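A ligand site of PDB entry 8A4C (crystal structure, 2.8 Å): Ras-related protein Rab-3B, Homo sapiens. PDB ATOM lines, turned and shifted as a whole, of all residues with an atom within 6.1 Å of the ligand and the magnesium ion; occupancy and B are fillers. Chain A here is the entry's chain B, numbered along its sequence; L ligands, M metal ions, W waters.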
ATOM      1  N   GLY A  31      33.031  22.771  -5.936  1.00  0.00           N
ATOM      2  CA  GLY A  31      33.548  22.640  -4.576  1.00  0.00           C
ATOM      3  C   GLY A  31      32.681  21.703  -3.759  1.00  0.00           C
ATOM      4  O   GLY A  31      31.646  21.247  -4.256  1.00  0.00           O
ATOM      5  N   ASN A  32      33.073  21.433  -2.516  1.00  0.00           N
ATOM      6  CA  ASN A  32      32.434  20.419  -1.679  1.00  0.00           C
ATOM      7  C   ASN A  32      31.009  20.835  -1.316  1.00  0.00           C
ATOM      8  O   ASN A  32      30.584  21.963  -1.525  1.00  0.00           O
ATOM      9  CB  ASN A  32      33.246  20.195  -0.406  1.00  0.00           C
ATOM     10  CG  ASN A  32      34.400  19.233  -0.609  1.00  0.00           C
ATOM     11  OD1 ASN A  32      34.804  18.944  -1.738  1.00  0.00           O
ATOM     12  ND2 ASN A  32      34.969  18.758   0.491  1.00  0.00           N
ATOM     13  N   SER A  33      30.252  19.877  -0.777  1.00  0.00           N
ATOM     14  CA  SER A  33      28.912  20.182  -0.309  1.00  0.00           C
ATOM     15  C   SER A  33      28.982  21.094   0.915  1.00  0.00           C
ATOM     16  O   SER A  33      29.945  21.045   1.683  1.00  0.00           O
ATOM     17  CB  SER A  33      28.152  18.892  -0.002  1.00  0.00           C
ATOM     18  OG  SER A  33      26.765  19.123   0.155  1.00  0.00           O
ATOM     19  N   SER A  34      27.979  21.976   1.036  1.00  0.00           N
ATOM     20  CA  SER A  34      27.739  22.935   2.128  1.00  0.00           C
ATOM     21  C   SER A  34      28.739  24.090   2.177  1.00  0.00           C
ATOM     22  O   SER A  34      28.792  24.807   3.182  1.00  0.00           O
ATOM     23  CB  SER A  34      27.702  22.258   3.506  1.00  0.00           C
ATOM     24  OG  SER A  34      26.638  21.325   3.577  1.00  0.00           O
ATOM     25  N   VAL A  35      29.521  24.339   1.124  1.00  0.00           N
ATOM     26  CA  VAL A  35      30.409  25.490   1.166  1.00  0.00           C
ATOM     27  C   VAL A  35      29.717  26.796   0.773  1.00  0.00           C
ATOM     28  O   VAL A  35      30.257  27.874   1.038  1.00  0.00           O
ATOM     29  CB  VAL A  35      31.641  25.269   0.273  1.00  0.00           C
ATOM     30  CG1 VAL A  35      32.414  24.058   0.740  1.00  0.00           C
ATOM     31  CG2 VAL A  35      31.208  25.088  -1.157  1.00  0.00           C
ATOM     32  N   GLY A  36      28.538  26.726   0.143  1.00  0.00           N
ATOM     33  CA  GLY A  36      27.774  27.923  -0.164  1.00  0.00           C
ATOM     34  C   GLY A  36      27.662  28.277  -1.643  1.00  0.00           C
ATOM     35  O   GLY A  36      27.522  29.451  -1.976  1.00  0.00           O
ATOM     36  N   LYS A  37      27.706  27.267  -2.512  1.00  0.00           N
ATOM     37  CA  LYS A  37      27.763  27.529  -3.956  1.00  0.00           C
ATOM     38  C   LYS A  37      26.438  28.081  -4.481  1.00  0.00           C
ATOM     39  O   LYS A  37      26.422  29.066  -5.241  1.00  0.00           O
ATOM     40  CB  LYS A  37      28.136  26.241  -4.697  1.00  0.00           C
ATOM     41  CG  LYS A  37      29.527  25.742  -4.354  1.00  0.00           C
ATOM     42  CD  LYS A  37      29.921  24.528  -5.175  1.00  0.00           C
ATOM     43  CE  LYS A  37      29.040  23.349  -4.879  1.00  0.00           C
ATOM     44  NZ  LYS A  37      29.079  23.008  -3.435  1.00  0.00           N
ATOM     45  N   THR A  38      25.330  27.454  -4.092  1.00  0.00           N
ATOM     46  CA  THR A  38      24.006  27.934  -4.466  1.00  0.00           C
ATOM     47  C   THR A  38      23.726  29.311  -3.876  1.00  0.00           C
ATOM     48  O   THR A  38      23.213  30.195  -4.573  1.00  0.00           O
ATOM     49  CB  THR A  38      22.960  26.928  -3.995  1.00  0.00           C
ATOM     50  OG1 THR A  38      23.248  25.653  -4.569  1.00  0.00           O
ATOM     51  CG2 THR A  38      21.559  27.336  -4.393  1.00  0.00           C
ATOM     52  N   SER A  39      24.101  29.512  -2.605  1.00  0.00           N
ATOM     53  CA  SER A  39      23.958  30.806  -1.952  1.00  0.00           C
ATOM     54  C   SER A  39      24.782  31.878  -2.639  1.00  0.00           C
ATOM     55  O   SER A  39      24.332  33.023  -2.790  1.00  0.00           O
ATOM     56  CB  SER A  39      24.364  30.688  -0.484  1.00  0.00           C
ATOM     57  OG  SER A  39      23.554  29.736   0.195  1.00  0.00           O
ATOM     58  N   PHE A  40      25.999  31.519  -3.087  1.00  0.00           N
ATOM     59  CA  PHE A  40      26.836  32.440  -3.843  1.00  0.00           C
ATOM     60  C   PHE A  40      26.176  32.862  -5.150  1.00  0.00           C
ATOM     61  O   PHE A  40      26.155  34.057  -5.499  1.00  0.00           O
ATOM     62  CB  PHE A  40      28.181  31.779  -4.144  1.00  0.00           C
ATOM     63  CG  PHE A  40      29.331  32.733  -4.188  1.00  0.00           C
ATOM     64  CD1 PHE A  40      29.875  33.230  -3.014  1.00  0.00           C
ATOM     65  CD2 PHE A  40      29.894  33.115  -5.400  1.00  0.00           C
ATOM     66  CE1 PHE A  40      30.941  34.110  -3.039  1.00  0.00           C
ATOM     67  CE2 PHE A  40      30.968  33.995  -5.430  1.00  0.00           C
ATOM     68  CZ  PHE A  40      31.490  34.486  -4.253  1.00  0.00           C
ATOM     69  N   PHE A  49      19.608  36.415   0.212  1.00  0.00           N
ATOM     70  CA  PHE A  49      20.139  35.264   0.931  1.00  0.00           C
ATOM     71  C   PHE A  49      19.048  34.698   1.840  1.00  0.00           C
ATOM     72  O   PHE A  49      18.431  35.447   2.600  1.00  0.00           O
ATOM     73  CB  PHE A  49      21.372  35.640   1.750  1.00  0.00           C
ATOM     74  CG  PHE A  49      21.978  34.489   2.511  1.00  0.00           C
ATOM     75  CD1 PHE A  49      22.881  33.645   1.893  1.00  0.00           C
ATOM     76  CD2 PHE A  49      21.682  34.272   3.856  1.00  0.00           C
ATOM     77  CE1 PHE A  49      23.458  32.584   2.574  1.00  0.00           C
ATOM     78  CE2 PHE A  49      22.232  33.217   4.551  1.00  0.00           C
ATOM     79  CZ  PHE A  49      23.133  32.367   3.911  1.00  0.00           C
ATOM     80  N   THR A  50      18.853  33.378   1.790  1.00  0.00           N
ATOM     81  CA  THR A  50      18.014  32.672   2.742  1.00  0.00           C
ATOM     82  C   THR A  50      18.842  31.625   3.479  1.00  0.00           C
ATOM     83  O   THR A  50      19.666  30.947   2.852  1.00  0.00           O
ATOM     84  CB  THR A  50      16.820  31.976   2.056  1.00  0.00           C
ATOM     85  OG1 THR A  50      17.284  30.827   1.340  1.00  0.00           O
ATOM     86  CG2 THR A  50      16.104  32.920   1.098  1.00  0.00           C
ATOM     87  N   PRO A  51      18.650  31.475   4.796  1.00  0.00           N
ATOM     88  CA  PRO A  51      19.443  30.469   5.525  1.00  0.00           C
ATOM     89  C   PRO A  51      19.020  29.032   5.264  1.00  0.00           C
ATOM     90  O   PRO A  51      19.724  28.109   5.728  1.00  0.00           O
ATOM     91  CB  PRO A  51      19.228  30.840   7.001  1.00  0.00           C
ATOM     92  CG  PRO A  51      18.369  32.044   7.030  1.00  0.00           C
ATOM     93  CD  PRO A  51      17.869  32.349   5.664  1.00  0.00           C
ATOM     94  N   ALA A  52      17.922  28.804   4.539  1.00  0.00           N
ATOM     95  CA  ALA A  52      17.391  27.468   4.300  1.00  0.00           C
ATOM     96  C   ALA A  52      18.324  26.676   3.409  1.00  0.00           C
ATOM     97  O   ALA A  52      18.437  26.945   2.200  1.00  0.00           O
ATOM     98  CB  ALA A  52      15.997  27.570   3.677  1.00  0.00           C
ATOM     99  N   PHE A  53      19.004  25.688   3.987  1.00  0.00           N
ATOM    100  CA  PHE A  53      19.897  24.791   3.248  1.00  0.00           C
ATOM    101  C   PHE A  53      19.053  23.765   2.490  1.00  0.00           C
ATOM    102  O   PHE A  53      18.440  22.878   3.100  1.00  0.00           O
ATOM    103  CB  PHE A  53      20.865  24.105   4.211  1.00  0.00           C
ATOM    104  CG  PHE A  53      21.858  23.151   3.559  1.00  0.00           C
ATOM    105  CD1 PHE A  53      22.288  23.319   2.242  1.00  0.00           C
ATOM    106  CD2 PHE A  53      22.382  22.085   4.286  1.00  0.00           C
ATOM    107  CE1 PHE A  53      23.206  22.433   1.656  1.00  0.00           C
ATOM    108  CE2 PHE A  53      23.296  21.201   3.713  1.00  0.00           C
ATOM    109  CZ  PHE A  53      23.702  21.373   2.397  1.00  0.00           C
ATOM    110  N   VAL A  54      19.043  23.864   1.165  1.00  0.00           N
ATOM    111  CA  VAL A  54      18.636  22.763   0.302  1.00  0.00           C
ATOM    112  C   VAL A  54      19.814  22.403  -0.614  1.00  0.00           C
ATOM    113  O   VAL A  54      20.418  23.269  -1.259  1.00  0.00           O
ATOM    114  CB  VAL A  54      17.332  23.072  -0.469  1.00  0.00           C
ATOM    115  CG1 VAL A  54      17.447  24.276  -1.383  1.00  0.00           C
ATOM    116  CG2 VAL A  54      16.902  21.842  -1.266  1.00  0.00           C
ATOM    117  N   SER A  55      20.179  21.125  -0.605  1.00  0.00           N
ATOM    118  CA  SER A  55      21.347  20.701  -1.366  1.00  0.00           C
ATOM    119  C   SER A  55      20.966  20.570  -2.834  1.00  0.00           C
ATOM    120  O   SER A  55      19.879  20.073  -3.161  1.00  0.00           O
ATOM    121  CB  SER A  55      21.879  19.384  -0.813  1.00  0.00           C
ATOM    122  OG  SER A  55      23.187  19.110  -1.287  1.00  0.00           O
ATOM    123  N   THR A  56      21.852  21.028  -3.714  1.00  0.00           N
ATOM    124  CA  THR A  56      21.594  20.942  -5.149  1.00  0.00           C
ATOM    125  C   THR A  56      21.651  19.487  -5.600  1.00  0.00           C
ATOM    126  O   THR A  56      22.556  18.735  -5.213  1.00  0.00           O
ATOM    127  CB  THR A  56      22.609  21.782  -5.928  1.00  0.00           C
ATOM    128  OG1 THR A  56      22.634  23.116  -5.415  1.00  0.00           O
ATOM    129  CG2 THR A  56      22.259  21.838  -7.416  1.00  0.00           C
ATOM    130  N   VAL A  57      20.666  19.077  -6.379  1.00  0.00           N
ATOM    131  CA  VAL A  57      20.644  17.753  -6.996  1.00  0.00           C
ATOM    132  C   VAL A  57      21.132  17.912  -8.429  1.00  0.00           C
ATOM    133  O   VAL A  57      20.475  18.562  -9.253  1.00  0.00           O
ATOM    134  CB  VAL A  57      19.250  17.132  -6.955  1.00  0.00           C
ATOM    135  CG1 VAL A  57      19.275  15.775  -7.637  1.00  0.00           C
ATOM    136  CG2 VAL A  57      18.755  17.014  -5.523  1.00  0.00           C
ATOM    137  N   ASP A  79      25.804  26.243 -11.230  1.00  0.00           N
ATOM    138  CA  ASP A  79      25.992  25.780  -9.862  1.00  0.00           C
ATOM    139  C   ASP A  79      26.038  24.245  -9.905  1.00  0.00           C
ATOM    140  O   ASP A  79      25.057  23.610 -10.323  1.00  0.00           O
ATOM    141  CB  ASP A  79      24.811  26.270  -9.033  1.00  0.00           C
ATOM    142  CG  ASP A  79      24.827  25.773  -7.587  1.00  0.00           C
ATOM    143  OD1 ASP A  79      25.840  25.238  -7.094  1.00  0.00           O
ATOM    144  OD2 ASP A  79      23.737  25.822  -6.978  1.00  0.00           O
ATOM    145  N   THR A  80      27.153  23.652  -9.472  1.00  0.00           N
ATOM    146  CA  THR A  80      27.229  22.199  -9.431  1.00  0.00           C
ATOM    147  C   THR A  80      26.863  21.693  -8.039  1.00  0.00           C
ATOM    148  O   THR A  80      26.773  22.454  -7.078  1.00  0.00           O
ATOM    149  CB  THR A  80      28.633  21.721  -9.805  1.00  0.00           C
ATOM    150  OG1 THR A  80      29.576  22.277  -8.889  1.00  0.00           O
ATOM    151  CG2 THR A  80      28.967  22.150 -11.208  1.00  0.00           C
ATOM    152  N   ALA A  81      26.651  20.379  -7.947  1.00  0.00           N
ATOM    153  CA  ALA A  81      26.418  19.729  -6.660  1.00  0.00           C
ATOM    154  C   ALA A  81      27.732  19.206  -6.090  1.00  0.00           C
ATOM    155  O   ALA A  81      28.549  18.631  -6.817  1.00  0.00           O
ATOM    156  CB  ALA A  81      25.413  18.582  -6.808  1.00  0.00           C
ATOM    157  N   GLY A  82      27.931  19.414  -4.792  1.00  0.00           N
ATOM    158  CA  GLY A  82      29.180  19.029  -4.142  1.00  0.00           C
ATOM    159  C   GLY A  82      29.258  17.580  -3.709  1.00  0.00           C
ATOM    160  O   GLY A  82      30.363  17.089  -3.472  1.00  0.00           O
ATOM    161  N   GLN A  83      28.123  16.892  -3.598  1.00  0.00           N
ATOM    162  CA  GLN A  83      28.102  15.502  -3.156  1.00  0.00           C
ATOM    163  C   GLN A  83      28.773  14.608  -4.197  1.00  0.00           C
ATOM    164  O   GLN A  83      28.746  14.880  -5.398  1.00  0.00           O
ATOM    165  CB  GLN A  83      26.667  15.031  -2.920  1.00  0.00           C
ATOM    166  CG  GLN A  83      25.938  15.747  -1.786  1.00  0.00           C
ATOM    167  CD  GLN A  83      24.487  15.314  -1.641  1.00  0.00           C
ATOM    168  OE1 GLN A  83      24.142  14.156  -1.903  1.00  0.00           O
ATOM    169  NE2 GLN A  83      23.624  16.238  -1.239  1.00  0.00           N
ATOM    170  N   ASN A 137      34.450  30.946   1.134  1.00  0.00           N
ATOM    171  CA  ASN A 137      33.176  31.484   1.555  1.00  0.00           C
ATOM    172  C   ASN A 137      33.064  31.482   3.084  1.00  0.00           C
ATOM    173  O   ASN A 137      33.886  30.907   3.793  1.00  0.00           O
ATOM    174  CB  ASN A 137      32.040  30.670   0.931  1.00  0.00           C
ATOM    175  CG  ASN A 137      30.733  31.448   0.856  1.00  0.00           C
ATOM    176  OD1 ASN A 137      30.729  32.678   0.912  1.00  0.00           O
ATOM    177  ND2 ASN A 137      29.606  30.734   0.752  1.00  0.00           N
ATOM    178  N   LYS A 138      32.016  32.174   3.555  1.00  0.00           N
ATOM    179  CA  LYS A 138      31.603  32.278   4.961  1.00  0.00           C
ATOM    180  C   LYS A 138      32.629  33.043   5.792  1.00  0.00           C
ATOM    181  O   LYS A 138      32.880  32.701   6.951  1.00  0.00           O
ATOM    182  CB  LYS A 138      31.284  30.914   5.579  1.00  0.00           C
ATOM    183  CG  LYS A 138      30.306  30.077   4.749  1.00  0.00           C
ATOM    184  CD  LYS A 138      29.827  28.869   5.509  1.00  0.00           C
ATOM    185  CE  LYS A 138      29.035  27.941   4.594  1.00  0.00           C
ATOM    186  NZ  LYS A 138      28.576  26.733   5.330  1.00  0.00           N
ATOM    187  N   CYS A 139      33.190  34.104   5.216  1.00  0.00           N
ATOM    188  CA  CYS A 139      34.150  34.915   5.956  1.00  0.00           C
ATOM    189  C   CYS A 139      33.482  35.775   7.033  1.00  0.00           C
ATOM    190  O   CYS A 139      34.192  36.321   7.881  1.00  0.00           O
ATOM    191  CB  CYS A 139      34.979  35.778   5.008  1.00  0.00           C
ATOM    192  SG  CYS A 139      34.192  37.267   4.325  1.00  0.00           S
ATOM    193  N   ASP A 140      32.152  35.877   7.025  1.00  0.00           N
ATOM    194  CA  ASP A 140      31.427  36.483   8.139  1.00  0.00           C
ATOM    195  C   ASP A 140      31.505  35.646   9.417  1.00  0.00           C
ATOM    196  O   ASP A 140      31.274  36.189  10.500  1.00  0.00           O
ATOM    197  CB  ASP A 140      29.949  36.673   7.776  1.00  0.00           C
ATOM    198  CG  ASP A 140      29.262  35.372   7.381  1.00  0.00           C
ATOM    199  OD1 ASP A 140      29.681  34.744   6.382  1.00  0.00           O
ATOM    200  OD2 ASP A 140      28.306  34.967   8.072  1.00  0.00           O
ATOM    201  N   MET A 141      31.816  34.355   9.303  1.00  0.00           N
ATOM    202  CA  MET A 141      31.825  33.459  10.460  1.00  0.00           C
ATOM    203  C   MET A 141      33.244  33.369  11.014  1.00  0.00           C
ATOM    204  O   MET A 141      33.911  32.330  10.970  1.00  0.00           O
ATOM    205  CB  MET A 141      31.282  32.095  10.068  1.00  0.00           C
ATOM    206  CG  MET A 141      29.830  32.131   9.654  1.00  0.00           C
ATOM    207  SD  MET A 141      28.703  32.211  11.046  1.00  0.00           S
ATOM    208  CE  MET A 141      28.812  30.529  11.677  1.00  0.00           C
ATOM    209  N   ALA A 166      35.003  35.538   0.862  1.00  0.00           N
ATOM    210  CA  ALA A 166      33.711  36.092   0.537  1.00  0.00           C
ATOM    211  C   ALA A 166      32.670  35.628   1.547  1.00  0.00           C
ATOM    212  O   ALA A 166      32.911  34.760   2.384  1.00  0.00           O
ATOM    213  CB  ALA A 166      33.296  35.696  -0.878  1.00  0.00           C
ATOM    214  N   SER A 167      31.505  36.251   1.451  1.00  0.00           N
ATOM    215  CA  SER A 167      30.358  35.881   2.264  1.00  0.00           C
ATOM    216  C   SER A 167      29.105  36.047   1.410  1.00  0.00           C
ATOM    217  O   SER A 167      28.715  37.176   1.107  1.00  0.00           O
ATOM    218  CB  SER A 167      30.269  36.721   3.524  1.00  0.00           C
ATOM    219  OG  SER A 167      29.081  36.400   4.231  1.00  0.00           O
ATOM    220  N   ALA A 168      28.482  34.921   1.041  1.00  0.00           N
ATOM    221  CA  ALA A 168      27.203  34.970   0.360  1.00  0.00           C
ATOM    222  C   ALA A 168      26.109  35.542   1.251  1.00  0.00           C
ATOM    223  O   ALA A 168      25.146  36.134   0.754  1.00  0.00           O
ATOM    224  CB  ALA A 168      26.822  33.569  -0.125  1.00  0.00           C
ATOM    225  N   LYS A 169      26.239  35.362   2.575  1.00  0.00           N
ATOM    226  CA  LYS A 169      25.249  35.870   3.517  1.00  0.00           C
ATOM    227  C   LYS A 169      25.284  37.387   3.607  1.00  0.00           C
ATOM    228  O   LYS A 169      24.236  38.042   3.588  1.00  0.00           O
ATOM    229  CB  LYS A 169      25.489  35.253   4.893  1.00  0.00           C
ATOM    230  CG  LYS A 169      24.487  35.665   5.942  1.00  0.00           C
ATOM    231  CD  LYS A 169      24.438  34.661   7.079  1.00  0.00           C
ATOM    232  CE  LYS A 169      23.557  35.152   8.222  1.00  0.00           C
ATOM    233  NZ  LYS A 169      24.265  35.119   9.528  1.00  0.00           N
ATOM    234  N   GLU A 170      26.478  37.971   3.711  1.00  0.00           N
ATOM    235  CA  GLU A 170      26.618  39.396   3.960  1.00  0.00           C
ATOM    236  C   GLU A 170      27.031  40.198   2.727  1.00  0.00           C
ATOM    237  O   GLU A 170      27.262  41.409   2.862  1.00  0.00           O
ATOM    238  CB  GLU A 170      27.638  39.628   5.085  1.00  0.00           C
ATOM    239  CG  GLU A 170      27.394  38.821   6.355  1.00  0.00           C
ATOM    240  CD  GLU A 170      26.133  39.221   7.132  1.00  0.00           C
ATOM    241  OE1 GLU A 170      25.537  40.290   6.888  1.00  0.00           O
ATOM    242  OE2 GLU A 170      25.732  38.416   8.014  1.00  0.00           O
HETATM  243  P1  LIG L   1      25.598  21.545  -2.342  1.00  0.00           P
HETATM  244  O1  LIG L   1      24.447  21.874  -3.224  1.00  0.00           O
HETATM  245  O2  LIG L   1      26.888  21.486  -3.163  1.00  0.00           O
HETATM  246  O3  LIG L   1      25.350  20.176  -1.652  1.00  0.00           O
HETATM  247  N1  LIG L   1      25.714  22.753  -1.143  1.00  0.00           N
HETATM  248  P2  LIG L   1      26.140  24.281  -1.559  1.00  0.00           P
HETATM  249  O4  LIG L   1      27.589  24.340  -1.980  1.00  0.00           O
HETATM  250  O5  LIG L   1      25.265  24.754  -2.687  1.00  0.00           O
HETATM  251  O6  LIG L   1      25.927  25.218  -0.228  1.00  0.00           O
HETATM  252  P3  LIG L   1      24.597  26.071   0.049  1.00  0.00           P
HETATM  253  O7  LIG L   1      24.618  27.253  -0.923  1.00  0.00           O
HETATM  254  O8  LIG L   1      23.378  25.252  -0.020  1.00  0.00           O
HETATM  255  O9  LIG L   1      24.845  26.559   1.524  1.00  0.00           O
HETATM  256  C1  LIG L   1      25.015  25.618   2.605  1.00  0.00           C
HETATM  257  C2  LIG L   1      24.687  26.252   3.930  1.00  0.00           C
HETATM  258  O10 LIG L   1      25.653  27.277   4.248  1.00  0.00           O
HETATM  259  C3  LIG L   1      23.309  26.916   4.053  1.00  0.00           C
HETATM  260  O11 LIG L   1      22.747  26.668   5.333  1.00  0.00           O
HETATM  261  C4  LIG L   1      23.624  28.409   3.864  1.00  0.00           C
HETATM  262  O12 LIG L   1      22.698  29.224   4.570  1.00  0.00           O
HETATM  263  C5  LIG L   1      25.014  28.510   4.492  1.00  0.00           C
HETATM  264  N2  LIG L   1      25.835  29.580   3.894  1.00  0.00           N
HETATM  265  C6  LIG L   1      26.131  29.739   2.573  1.00  0.00           C
HETATM  266  N3  LIG L   1      26.903  30.781   2.336  1.00  0.00           N
HETATM  267  C7  LIG L   1      27.114  31.335   3.585  1.00  0.00           C
HETATM  268  C8  LIG L   1      27.859  32.498   4.002  1.00  0.00           C
HETATM  269  O13 LIG L   1      28.499  33.275   3.297  1.00  0.00           O
HETATM  270  N4  LIG L   1      27.821  32.684   5.374  1.00  0.00           N
HETATM  271  C9  LIG L   1      27.137  31.889   6.247  1.00  0.00           C
HETATM  272  N5  LIG L   1      27.194  32.225   7.540  1.00  0.00           N
HETATM  273  N6  LIG L   1      26.440  30.818   5.888  1.00  0.00           N
HETATM  274  C10 LIG L   1      26.462  30.605   4.560  1.00  0.00           C
HETATM  275 MG    MG M   1      23.773  23.672  -3.828  1.00  0.00          MG
HETATM  276  O   HOH W   1      25.481  23.728  -5.015  1.00  0.00           O
HETATM  277  O   HOH W   2      24.298  29.819   7.911  1.00  0.00           O
HETATM  278  O   HOH W   3      22.471  24.297  -2.061  1.00  0.00           O
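OD2 of Asp 79 touches the magnesium ion, 3.8 Å away. The nearest printed residue that does not touch the magnesium ion is Val 54 (4.2 Å).
N of Ser 34 sits close to N1 of the ligand, 3.2 Å away. Asn 32 touches the ligand (O to O4, 3.9 Å). N of Val 35 touches O4 of the ligand (3.7 Å). Phe 49 touches the ligand. O of Thr 50 touches O12 of the ligand, 3.9 Å away. Phe 53 touches the ligand. Val 54 touches the ligand (O to O8, 3.8 Å). Ala 81 touches the ligand (C to O2, 3.8 Å). Met 141 touches the ligand (CG to N5, 3.4 Å). Hydrophobic or aromatic side chains within 4 Å of the ligand: Val 35, Phe 49, Phe 53, Met 141 and Ala 168. Within 4 Å of the ligand: Asn 32, Ser 33, Ser 34, Val 35, Gly 36, Lys 37, Thr 38, Ser 39, Phe 49, Thr 50, Pro 51, Phe 53, Val 54, Ser 55, Thr 56, Ala 81, Gly 82, Asn 137, Lys 138, Asp 140, Met 141, Ser 167, Ala 168 and Lys 169.
The magnesium ion is bound by an oxygen (O1) of the ligand, the side-chain hydroxyl (OG1) of Thr 56, water W1, an oxygen (O5) of the ligand, the side-chain hydroxyl (OG1) of Thr 38 and water W3.
Water W1 lies within hydrogen-bond range of the side-chain carboxylate (OD1) of Asp 79 (2.6 Å), the backbone carbonyl oxygen (O) of Thr 80 (2.7 Å) and an oxygen (O2) of the ligand (3.2 Å). Water W3 bridges an oxygen (O8) of the ligand (2.4 Å) and the backbone carbonyl oxygen of Val 54 (2.4 Å).
The backbone NH (N) of Thr 56 sits close to an oxygen (O1) of the ligand (2.8 Å). An oxygen (O4) of the ligand lies within salt-bridge range of the side-chain amino group of Lys 37 (2.5 Å). O13 of the ligand is in hydrogen-bond range of N of Lys 169 (3.2 Å). OG of Ser 39 lies within hydrogen-bond range of O7 of the ligand (2.9 Å). The backbone NH (N) of Ser 39 is in hydrogen-bond range of an oxygen (O7) of the ligand (2.9 Å). An oxygen (O4) of the ligand lies within hydrogen-bond range of the backbone NH of Lys 37, at 3.0 Å. An oxygen (O3) of the ligand is in hydrogen-bond range of the side-chain hydroxyl of Ser 55 (2.4 Å). OG of Ser 167 is in hydrogen-bond range of O13 of the ligand (3.3 Å). A nitrogen (N4) of the ligand is in hydrogen-bond range of the side-chain carboxylate of Asp 140. OG of Ser 33 lies within hydrogen-bond range of O3 of the ligand (2.5 Å). O2 of the ligand is in hydrogen-bond range of N of Gly 82, 2.8 Å away. ND2 of Asn 137 is in hydrogen-bond range of N3 of the ligand (3.1 Å). The backbone carbonyl oxygen (O) of Pro 51 lies within hydrogen-bond range of an oxygen (O11) of the ligand (3.4 Å). The backbone NH (N) of Ala 168 sits at hydrogen-bond distance from an oxygen (O13) of the ligand. NZ of Lys 138 is in hydrogen-bond range of O10 of the ligand. N of Thr 38 sits at hydrogen-bond distance from O7 of the ligand (3.3 Å). The backbone NH (N) of Gly 36 lies within hydrogen-bond range of an oxygen (O6) of the ligand, at 3.0 Å.
The backbone NH (N) of Lys 169 sits close to the side-chain hydroxyl (OG) of Ser 167 (3.4 Å). The side-chain carboxylate of Asp 140 sits at hydrogen-bond distance from the side-chain hydroxyl of Ser 167, 2.8 Å away. The side-chain hydroxyl (OG) of Ser 55 lies within hydrogen-bond range of the side-chain amide nitrogen (NE2) of Gln 83, 2.9 Å away. The side-chain hydroxyl of Thr 56 sits close to the side-chain carboxylate of Asp 79, at 3.3 Å. NZ of Lys 138 is in hydrogen-bond range of O of Ser 34, 2.9 Å away. The side-chain amino group of Lys 169 lies within salt-bridge range of the side-chain carboxylate of Glu 170, 3.9 Å away. ND2 of Asn 137 lies within hydrogen-bond range of O of Val 35 (2.9 Å). The backbone NH of Lys 138 sits at hydrogen-bond distance from the backbone carbonyl oxygen of Ala 166.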
